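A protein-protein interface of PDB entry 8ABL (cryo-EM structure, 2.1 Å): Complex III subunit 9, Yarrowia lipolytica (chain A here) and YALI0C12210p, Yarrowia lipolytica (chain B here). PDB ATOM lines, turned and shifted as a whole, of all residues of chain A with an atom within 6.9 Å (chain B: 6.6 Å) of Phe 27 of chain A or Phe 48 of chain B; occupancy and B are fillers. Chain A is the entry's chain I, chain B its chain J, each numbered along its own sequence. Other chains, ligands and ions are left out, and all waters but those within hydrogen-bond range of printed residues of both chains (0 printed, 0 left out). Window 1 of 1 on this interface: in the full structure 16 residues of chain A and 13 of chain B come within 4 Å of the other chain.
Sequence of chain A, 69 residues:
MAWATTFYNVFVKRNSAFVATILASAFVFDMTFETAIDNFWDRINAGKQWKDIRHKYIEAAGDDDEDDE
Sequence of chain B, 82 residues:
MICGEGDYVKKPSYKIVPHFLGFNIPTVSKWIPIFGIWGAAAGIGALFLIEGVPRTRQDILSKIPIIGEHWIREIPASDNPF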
ATOM      1  N   ILE A  22      -0.160   9.522 -27.828  1.00  0.00           N
ATOM      2  CA  ILE A  22      -1.382   9.131 -27.133  1.00  0.00           C
ATOM      3  C   ILE A  22      -1.749   7.689 -27.506  1.00  0.00           C
ATOM      4  O   ILE A  22      -2.063   6.894 -26.622  1.00  0.00           O
ATOM      5  CB  ILE A  22      -2.528  10.142 -27.395  1.00  0.00           C
ATOM      6  CG1 ILE A  22      -2.308  11.487 -26.686  1.00  0.00           C
ATOM      7  CG2 ILE A  22      -3.890   9.550 -27.056  1.00  0.00           C
ATOM      8  CD1 ILE A  22      -3.044  12.663 -27.329  1.00  0.00           C
ATOM      9  N   LEU A  23      -1.680   7.340 -28.802  1.00  0.00           N
ATOM     10  CA  LEU A  23      -2.067   6.003 -29.241  1.00  0.00           C
ATOM     11  C   LEU A  23      -1.085   4.951 -28.731  1.00  0.00           C
ATOM     12  O   LEU A  23      -1.519   3.892 -28.295  1.00  0.00           O
ATOM     13  CB  LEU A  23      -2.229   5.941 -30.762  1.00  0.00           C
ATOM     14  CG  LEU A  23      -3.385   6.774 -31.320  1.00  0.00           C
ATOM     15  CD1 LEU A  23      -3.434   6.724 -32.842  1.00  0.00           C
ATOM     16  CD2 LEU A  23      -4.721   6.358 -30.708  1.00  0.00           C
ATOM     17  N   ALA A  24       0.220   5.254 -28.748  1.00  0.00           N
ATOM     18  CA  ALA A  24       1.220   4.335 -28.216  1.00  0.00           C
ATOM     19  C   ALA A  24       0.999   4.114 -26.719  1.00  0.00           C
ATOM     20  O   ALA A  24       1.093   2.988 -26.241  1.00  0.00           O
ATOM     21  CB  ALA A  24       2.617   4.835 -28.499  1.00  0.00           C
ATOM     22  N   SER A  25       0.698   5.194 -25.993  1.00  0.00           N
ATOM     23  CA  SER A  25       0.398   5.123 -24.573  1.00  0.00           C
ATOM     24  C   SER A  25      -0.863   4.302 -24.322  1.00  0.00           C
ATOM     25  O   SER A  25      -0.921   3.556 -23.348  1.00  0.00           O
ATOM     26  CB  SER A  25       0.270   6.497 -23.989  1.00  0.00           C
ATOM     27  OG  SER A  25       1.445   7.241 -24.260  1.00  0.00           O
ATOM     28  N   ALA A  26      -1.870   4.454 -25.187  1.00  0.00           N
ATOM     29  CA  ALA A  26      -3.108   3.704 -25.021  1.00  0.00           C
ATOM     30  C   ALA A  26      -2.836   2.206 -25.155  1.00  0.00           C
ATOM     31  O   ALA A  26      -3.387   1.417 -24.394  1.00  0.00           O
ATOM     32  CB  ALA A  26      -4.165   4.184 -25.987  1.00  0.00           C
ATOM     33  N   PHE A  27      -1.981   1.840 -26.119  1.00  0.00           N
ATOM     34  CA  PHE A  27      -1.575   0.465 -26.364  1.00  0.00           C
ATOM     35  C   PHE A  27      -0.893  -0.105 -25.120  1.00  0.00           C
ATOM     36  O   PHE A  27      -1.272  -1.177 -24.650  1.00  0.00           O
ATOM     37  CB  PHE A  27      -0.662   0.411 -27.592  1.00  0.00           C
ATOM     38  CG  PHE A  27      -0.658  -0.892 -28.357  1.00  0.00           C
ATOM     39  CD1 PHE A  27      -0.803  -2.117 -27.712  1.00  0.00           C
ATOM     40  CD2 PHE A  27      -0.472  -0.896 -29.734  1.00  0.00           C
ATOM     41  CE1 PHE A  27      -0.791  -3.308 -28.426  1.00  0.00           C
ATOM     42  CE2 PHE A  27      -0.454  -2.087 -30.448  1.00  0.00           C
ATOM     43  CZ  PHE A  27      -0.613  -3.291 -29.795  1.00  0.00           C
ATOM     44  N   VAL A  28       0.069   0.640 -24.557  1.00  0.00           N
ATOM     45  CA  VAL A  28       0.815   0.188 -23.389  1.00  0.00           C
ATOM     46  C   VAL A  28      -0.129   0.089 -22.189  1.00  0.00           C
ATOM     47  O   VAL A  28      -0.123  -0.916 -21.479  1.00  0.00           O
ATOM     48  CB  VAL A  28       2.037   1.091 -23.117  1.00  0.00           C
ATOM     49  CG1 VAL A  28       2.736   0.770 -21.804  1.00  0.00           C
ATOM     50  CG2 VAL A  28       3.032   1.062 -24.271  1.00  0.00           C
ATOM     51  N   PHE A  29      -0.955   1.120 -21.980  1.00  0.00           N
ATOM     52  CA  PHE A  29      -1.920   1.109 -20.892  1.00  0.00           C
ATOM     53  C   PHE A  29      -2.779  -0.151 -20.972  1.00  0.00           C
ATOM     54  O   PHE A  29      -2.882  -0.890 -20.001  1.00  0.00           O
ATOM     55  CB  PHE A  29      -2.804   2.360 -20.908  1.00  0.00           C
ATOM     56  CG  PHE A  29      -3.945   2.285 -19.922  1.00  0.00           C
ATOM     57  CD1 PHE A  29      -3.740   2.586 -18.581  1.00  0.00           C
ATOM     58  CD2 PHE A  29      -5.207   1.855 -20.319  1.00  0.00           C
ATOM     59  CE1 PHE A  29      -4.780   2.492 -17.664  1.00  0.00           C
ATOM     60  CE2 PHE A  29      -6.247   1.758 -19.401  1.00  0.00           C
ATOM     61  CZ  PHE A  29      -6.031   2.078 -18.076  1.00  0.00           C
ATOM     62  N   ASP A  30      -3.386  -0.379 -22.137  1.00  0.00           N
ATOM     63  CA  ASP A  30      -4.274  -1.502 -22.386  1.00  0.00           C
ATOM     64  C   ASP A  30      -3.632  -2.832 -21.987  1.00  0.00           C
ATOM     65  O   ASP A  30      -4.287  -3.642 -21.342  1.00  0.00           O
ATOM     66  CB  ASP A  30      -4.705  -1.525 -23.852  1.00  0.00           C
ATOM     67  CG  ASP A  30      -6.005  -2.273 -24.090  1.00  0.00           C
ATOM     68  OD1 ASP A  30      -7.079  -1.710 -23.755  1.00  0.00           O
ATOM     69  OD2 ASP A  30      -5.950  -3.401 -24.619  1.00  0.00           O
ATOM     70  N   MET A  31      -2.369  -3.061 -22.369  1.00  0.00           N
ATOM     71  CA  MET A  31      -1.695  -4.323 -22.079  1.00  0.00           C
ATOM     72  C   MET A  31      -1.347  -4.456 -20.593  1.00  0.00           C
ATOM     73  O   MET A  31      -1.525  -5.525 -20.007  1.00  0.00           O
ATOM     74  CB  MET A  31      -0.438  -4.491 -22.938  1.00  0.00           C
ATOM     75  CG  MET A  31      -0.728  -4.453 -24.440  1.00  0.00           C
ATOM     76  SD  MET A  31      -1.855  -5.740 -25.070  1.00  0.00           S
ATOM     77  CE  MET A  31      -3.415  -4.863 -25.196  1.00  0.00           C
ATOM     78  N   THR A  32      -0.884  -3.369 -19.972  1.00  0.00           N
ATOM     79  CA  THR A  32      -0.427  -3.417 -18.591  1.00  0.00           C
ATOM     80  C   THR A  32      -1.623  -3.447 -17.651  1.00  0.00           C
ATOM     81  O   THR A  32      -1.603  -4.138 -16.643  1.00  0.00           O
ATOM     82  CB  THR A  32       0.540  -2.267 -18.297  1.00  0.00           C
ATOM     83  OG1 THR A  32      -0.169  -1.092 -18.690  1.00  0.00           O
ATOM     84  CG2 THR A  32       1.765  -2.370 -19.172  1.00  0.00           C
ATOM     85  N   GLY B  43      -0.428   3.545 -38.194  1.00  0.00           N
ATOM     86  CA  GLY B  43       0.079   2.194 -38.014  1.00  0.00           C
ATOM     87  C   GLY B  43      -0.139   1.685 -36.590  1.00  0.00           C
ATOM     88  O   GLY B  43      -0.722   0.617 -36.399  1.00  0.00           O
ATOM     89  N   ILE B  44       0.320   2.462 -35.600  1.00  0.00           N
ATOM     90  CA  ILE B  44       0.117   2.102 -34.204  1.00  0.00           C
ATOM     91  C   ILE B  44      -1.382   1.953 -33.950  1.00  0.00           C
ATOM     92  O   ILE B  44      -1.798   0.980 -33.334  1.00  0.00           O
ATOM     93  CB  ILE B  44       0.756   3.135 -33.255  1.00  0.00           C
ATOM     94  CG1 ILE B  44       2.279   3.191 -33.408  1.00  0.00           C
ATOM     95  CG2 ILE B  44       0.337   2.887 -31.813  1.00  0.00           C
ATOM     96  CD1 ILE B  44       2.899   4.516 -33.002  1.00  0.00           C
ATOM     97  N   GLY B  45      -2.178   2.918 -34.427  1.00  0.00           N
ATOM     98  CA  GLY B  45      -3.614   2.891 -34.180  1.00  0.00           C
ATOM     99  C   GLY B  45      -4.268   1.630 -34.747  1.00  0.00           C
ATOM    100  O   GLY B  45      -5.057   0.979 -34.063  1.00  0.00           O
ATOM    101  N   ALA B  46      -3.916   1.297 -35.999  1.00  0.00           N
ATOM    102  CA  ALA B  46      -4.511   0.186 -36.731  1.00  0.00           C
ATOM    103  C   ALA B  46      -4.153  -1.120 -36.029  1.00  0.00           C
ATOM    104  O   ALA B  46      -5.015  -1.957 -35.749  1.00  0.00           O
ATOM    105  CB  ALA B  46      -4.025   0.194 -38.163  1.00  0.00           C
ATOM    106  N   LEU B  47      -2.864  -1.245 -35.701  1.00  0.00           N
ATOM    107  CA  LEU B  47      -2.374  -2.446 -35.050  1.00  0.00           C
ATOM    108  C   LEU B  47      -3.041  -2.618 -33.688  1.00  0.00           C
ATOM    109  O   LEU B  47      -3.369  -3.737 -33.293  1.00  0.00           O
ATOM    110  CB  LEU B  47      -0.852  -2.369 -34.922  1.00  0.00           C
ATOM    111  CG  LEU B  47      -0.193  -3.551 -34.217  1.00  0.00           C
ATOM    112  CD1 LEU B  47      -0.263  -4.803 -35.082  1.00  0.00           C
ATOM    113  CD2 LEU B  47       1.253  -3.223 -33.879  1.00  0.00           C
ATOM    114  N   PHE B  48      -3.209  -1.505 -32.973  1.00  0.00           N
ATOM    115  CA  PHE B  48      -3.869  -1.543 -31.683  1.00  0.00           C
ATOM    116  C   PHE B  48      -5.315  -2.005 -31.848  1.00  0.00           C
ATOM    117  O   PHE B  48      -5.821  -2.726 -31.000  1.00  0.00           O
ATOM    118  CB  PHE B  48      -3.780  -0.165 -31.037  1.00  0.00           C
ATOM    119  CG  PHE B  48      -4.434  -0.030 -29.690  1.00  0.00           C
ATOM    120  CD1 PHE B  48      -4.227  -0.975 -28.689  1.00  0.00           C
ATOM    121  CD2 PHE B  48      -5.203   1.087 -29.398  1.00  0.00           C
ATOM    122  CE1 PHE B  48      -4.811  -0.819 -27.440  1.00  0.00           C
ATOM    123  CE2 PHE B  48      -5.781   1.245 -28.146  1.00  0.00           C
ATOM    124  CZ  PHE B  48      -5.586   0.290 -27.169  1.00  0.00           C
ATOM    125  N   LEU B  49      -5.970  -1.593 -32.940  1.00  0.00           N
ATOM    126  CA  LEU B  49      -7.367  -1.955 -33.146  1.00  0.00           C
ATOM    127  C   LEU B  49      -7.543  -3.453 -33.398  1.00  0.00           C
ATOM    128  O   LEU B  49      -8.618  -3.999 -33.154  1.00  0.00           O
ATOM    129  CB  LEU B  49      -7.962  -1.139 -34.293  1.00  0.00           C
ATOM    130  CG  LEU B  49      -8.509   0.230 -33.902  1.00  0.00           C
ATOM    131  CD1 LEU B  49      -8.928   0.997 -35.144  1.00  0.00           C
ATOM    132  CD2 LEU B  49      -9.684   0.099 -32.940  1.00  0.00           C
ATOM    133  N   ILE B  50      -6.511  -4.120 -33.912  1.00  0.00           N
ATOM    134  CA  ILE B  50      -6.677  -5.520 -34.267  1.00  0.00           C
ATOM    135  C   ILE B  50      -5.808  -6.373 -33.353  1.00  0.00           C
ATOM    136  O   ILE B  50      -5.510  -7.516 -33.676  1.00  0.00           O
ATOM    137  CB  ILE B  50      -6.348  -5.771 -35.753  1.00  0.00           C
ATOM    138  CG1 ILE B  50      -4.910  -5.354 -36.090  1.00  0.00           C
ATOM    139  CG2 ILE B  50      -7.389  -5.142 -36.675  1.00  0.00           C
ATOM    140  CD1 ILE B  50      -4.389  -5.900 -37.402  1.00  0.00           C
ATOM    141  N   GLU B  51      -5.399  -5.808 -32.217  1.00  0.00           N
ATOM    142  CA  GLU B  51      -4.539  -6.529 -31.297  1.00  0.00           C
ATOM    143  C   GLU B  51      -5.247  -7.788 -30.785  1.00  0.00           C
ATOM    144  O   GLU B  51      -4.598  -8.767 -30.445  1.00  0.00           O
ATOM    145  CB  GLU B  51      -4.095  -5.580 -30.184  1.00  0.00           C
ATOM    146  CG  GLU B  51      -3.408  -6.260 -29.004  1.00  0.00           C
ATOM    147  CD  GLU B  51      -4.262  -6.942 -27.936  1.00  0.00           C
ATOM    148  OE1 GLU B  51      -5.420  -6.511 -27.721  1.00  0.00           O
ATOM    149  OE2 GLU B  51      -3.762  -7.900 -27.300  1.00  0.00           O
ATOM    150  N   GLY B  52      -6.581  -7.756 -30.725  1.00  0.00           N
ATOM    151  CA  GLY B  52      -7.352  -8.899 -30.257  1.00  0.00           C
ATOM    152  C   GLY B  52      -7.422 -10.029 -31.286  1.00  0.00           C
ATOM    153  O   GLY B  52      -7.544 -11.195 -30.917  1.00  0.00           O
ATOM    154  N   LEU B  61       2.564  -9.791 -33.097  1.00  0.00           N
ATOM    155  CA  LEU B  61       2.813  -9.295 -31.752  1.00  0.00           C
ATOM    156  C   LEU B  61       3.662 -10.261 -30.934  1.00  0.00           C
ATOM    157  O   LEU B  61       4.444  -9.816 -30.102  1.00  0.00           O
ATOM    158  CB  LEU B  61       1.492  -8.988 -31.041  1.00  0.00           C
ATOM    159  CG  LEU B  61       0.701  -7.811 -31.606  1.00  0.00           C
ATOM    160  CD1 LEU B  61      -0.647  -7.677 -30.910  1.00  0.00           C
ATOM    161  CD2 LEU B  61       1.496  -6.515 -31.498  1.00  0.00           C
ATOM    162  N   TRP B  71       1.764 -12.197 -25.528  1.00  0.00           N
ATOM    163  CA  TRP B  71       0.704 -12.677 -26.407  1.00  0.00           C
ATOM    164  C   TRP B  71       0.777 -14.186 -26.643  1.00  0.00           C
ATOM    165  O   TRP B  71      -0.003 -14.718 -27.432  1.00  0.00           O
ATOM    166  CB  TRP B  71       0.652 -11.893 -27.727  1.00  0.00           C
ATOM    167  CG  TRP B  71       0.252 -10.458 -27.563  1.00  0.00           C
ATOM    168  CD1 TRP B  71      -1.013  -9.950 -27.471  1.00  0.00           C
ATOM    169  CD2 TRP B  71       1.141  -9.335 -27.454  1.00  0.00           C
ATOM    170  NE1 TRP B  71      -0.976  -8.588 -27.340  1.00  0.00           N
ATOM    171  CE2 TRP B  71       0.332  -8.183 -27.309  1.00  0.00           C
ATOM    172  CE3 TRP B  71       2.536  -9.191 -27.480  1.00  0.00           C
ATOM    173  CZ2 TRP B  71       0.877  -6.905 -27.199  1.00  0.00           C
ATOM    174  CZ3 TRP B  71       3.073  -7.928 -27.352  1.00  0.00           C
ATOM    175  CH2 TRP B  71       2.251  -6.804 -27.218  1.00  0.00           C
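The indole nitrogen of Trp 71 of chain B lies close to the side-chain sulfur of Met 31 of chain A (3.7 Å).
The side-chain carboxylate (OE2) of Glu 51 of chain B lies close to the side-chain sulfur (SD) of Met 31 of chain A (3.6 Å).
Of the printed residues of chain B, Leu 23 of chain A touches Ile 44 (3.97 Å).
Printed residues of chain B within 4 Å of Phe 27 of chain A: Leu 47 (3.997 Å), Phe 48 (3.6 Å) and Glu 51 (3.99 Å).
Printed residues of chain B within 4 Å of Met 31 of chain A: Glu 51 (3.5 Å) and Trp 71 (3.7 Å).
Gly 43 of chain B touches none of the printed residues of chain A.
Of the printed residues of chain A, Ile 44 of chain B touches Leu 23 and Ala 24.
Gly 45 of chain B touches none of the printed residues of chain A.
Of the printed residues of chain A, Leu 47 of chain B touches Phe 27 (3.997 Å).
Of chain A, only Ala 26 (3.7 Å), Phe 27 (3.6 Å) and Asp 30 (3.7 Å) come within 4 Å of Phe 48 of chain B.
The nearest printed residue of chain B that does not touch Phe 27 of chain A is Trp 71 of chain B (4.2 Å).
Among the printed residues, pairs that only touch across the chains: Phe 27 of chain A with Phe 48 of chain B (3.6 Å), Asp 30 of chain A with Phe 48 of chain B (3.7 Å), Ala 26 of chain A with Phe 48 of chain B (3.7 Å), Ala 24 of chain A with Ile 44 of chain B (3.9 Å), Leu 23 of chain A with Ile 44 of chain B (3.97 Å), Phe 27 of chain A with Glu 51 of chain B (3.99 Å) and Phe 27 of chain A with Leu 47 of chain B (3.997 Å).
Printed residues of chain B that touch a printed residue of chain A: Ile 44, Leu 47, Phe 48, Glu 51 and Trp 71.
Along chain B the printed residues that touch a printed residue of chain A span positions 44 to 71.
Of the 11 printed residues of chain A, 6 touch a printed residue of chain B.
Among the printed residues, no Asp or Glu carboxylate lies within 4 Å of a Lys or Arg side-chain nitrogen of the other chain.
NE1 of Trp 71 of chain B lies within hydrogen-bond range of OE2 of Glu 51 of chain B, 2.9 Å away.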
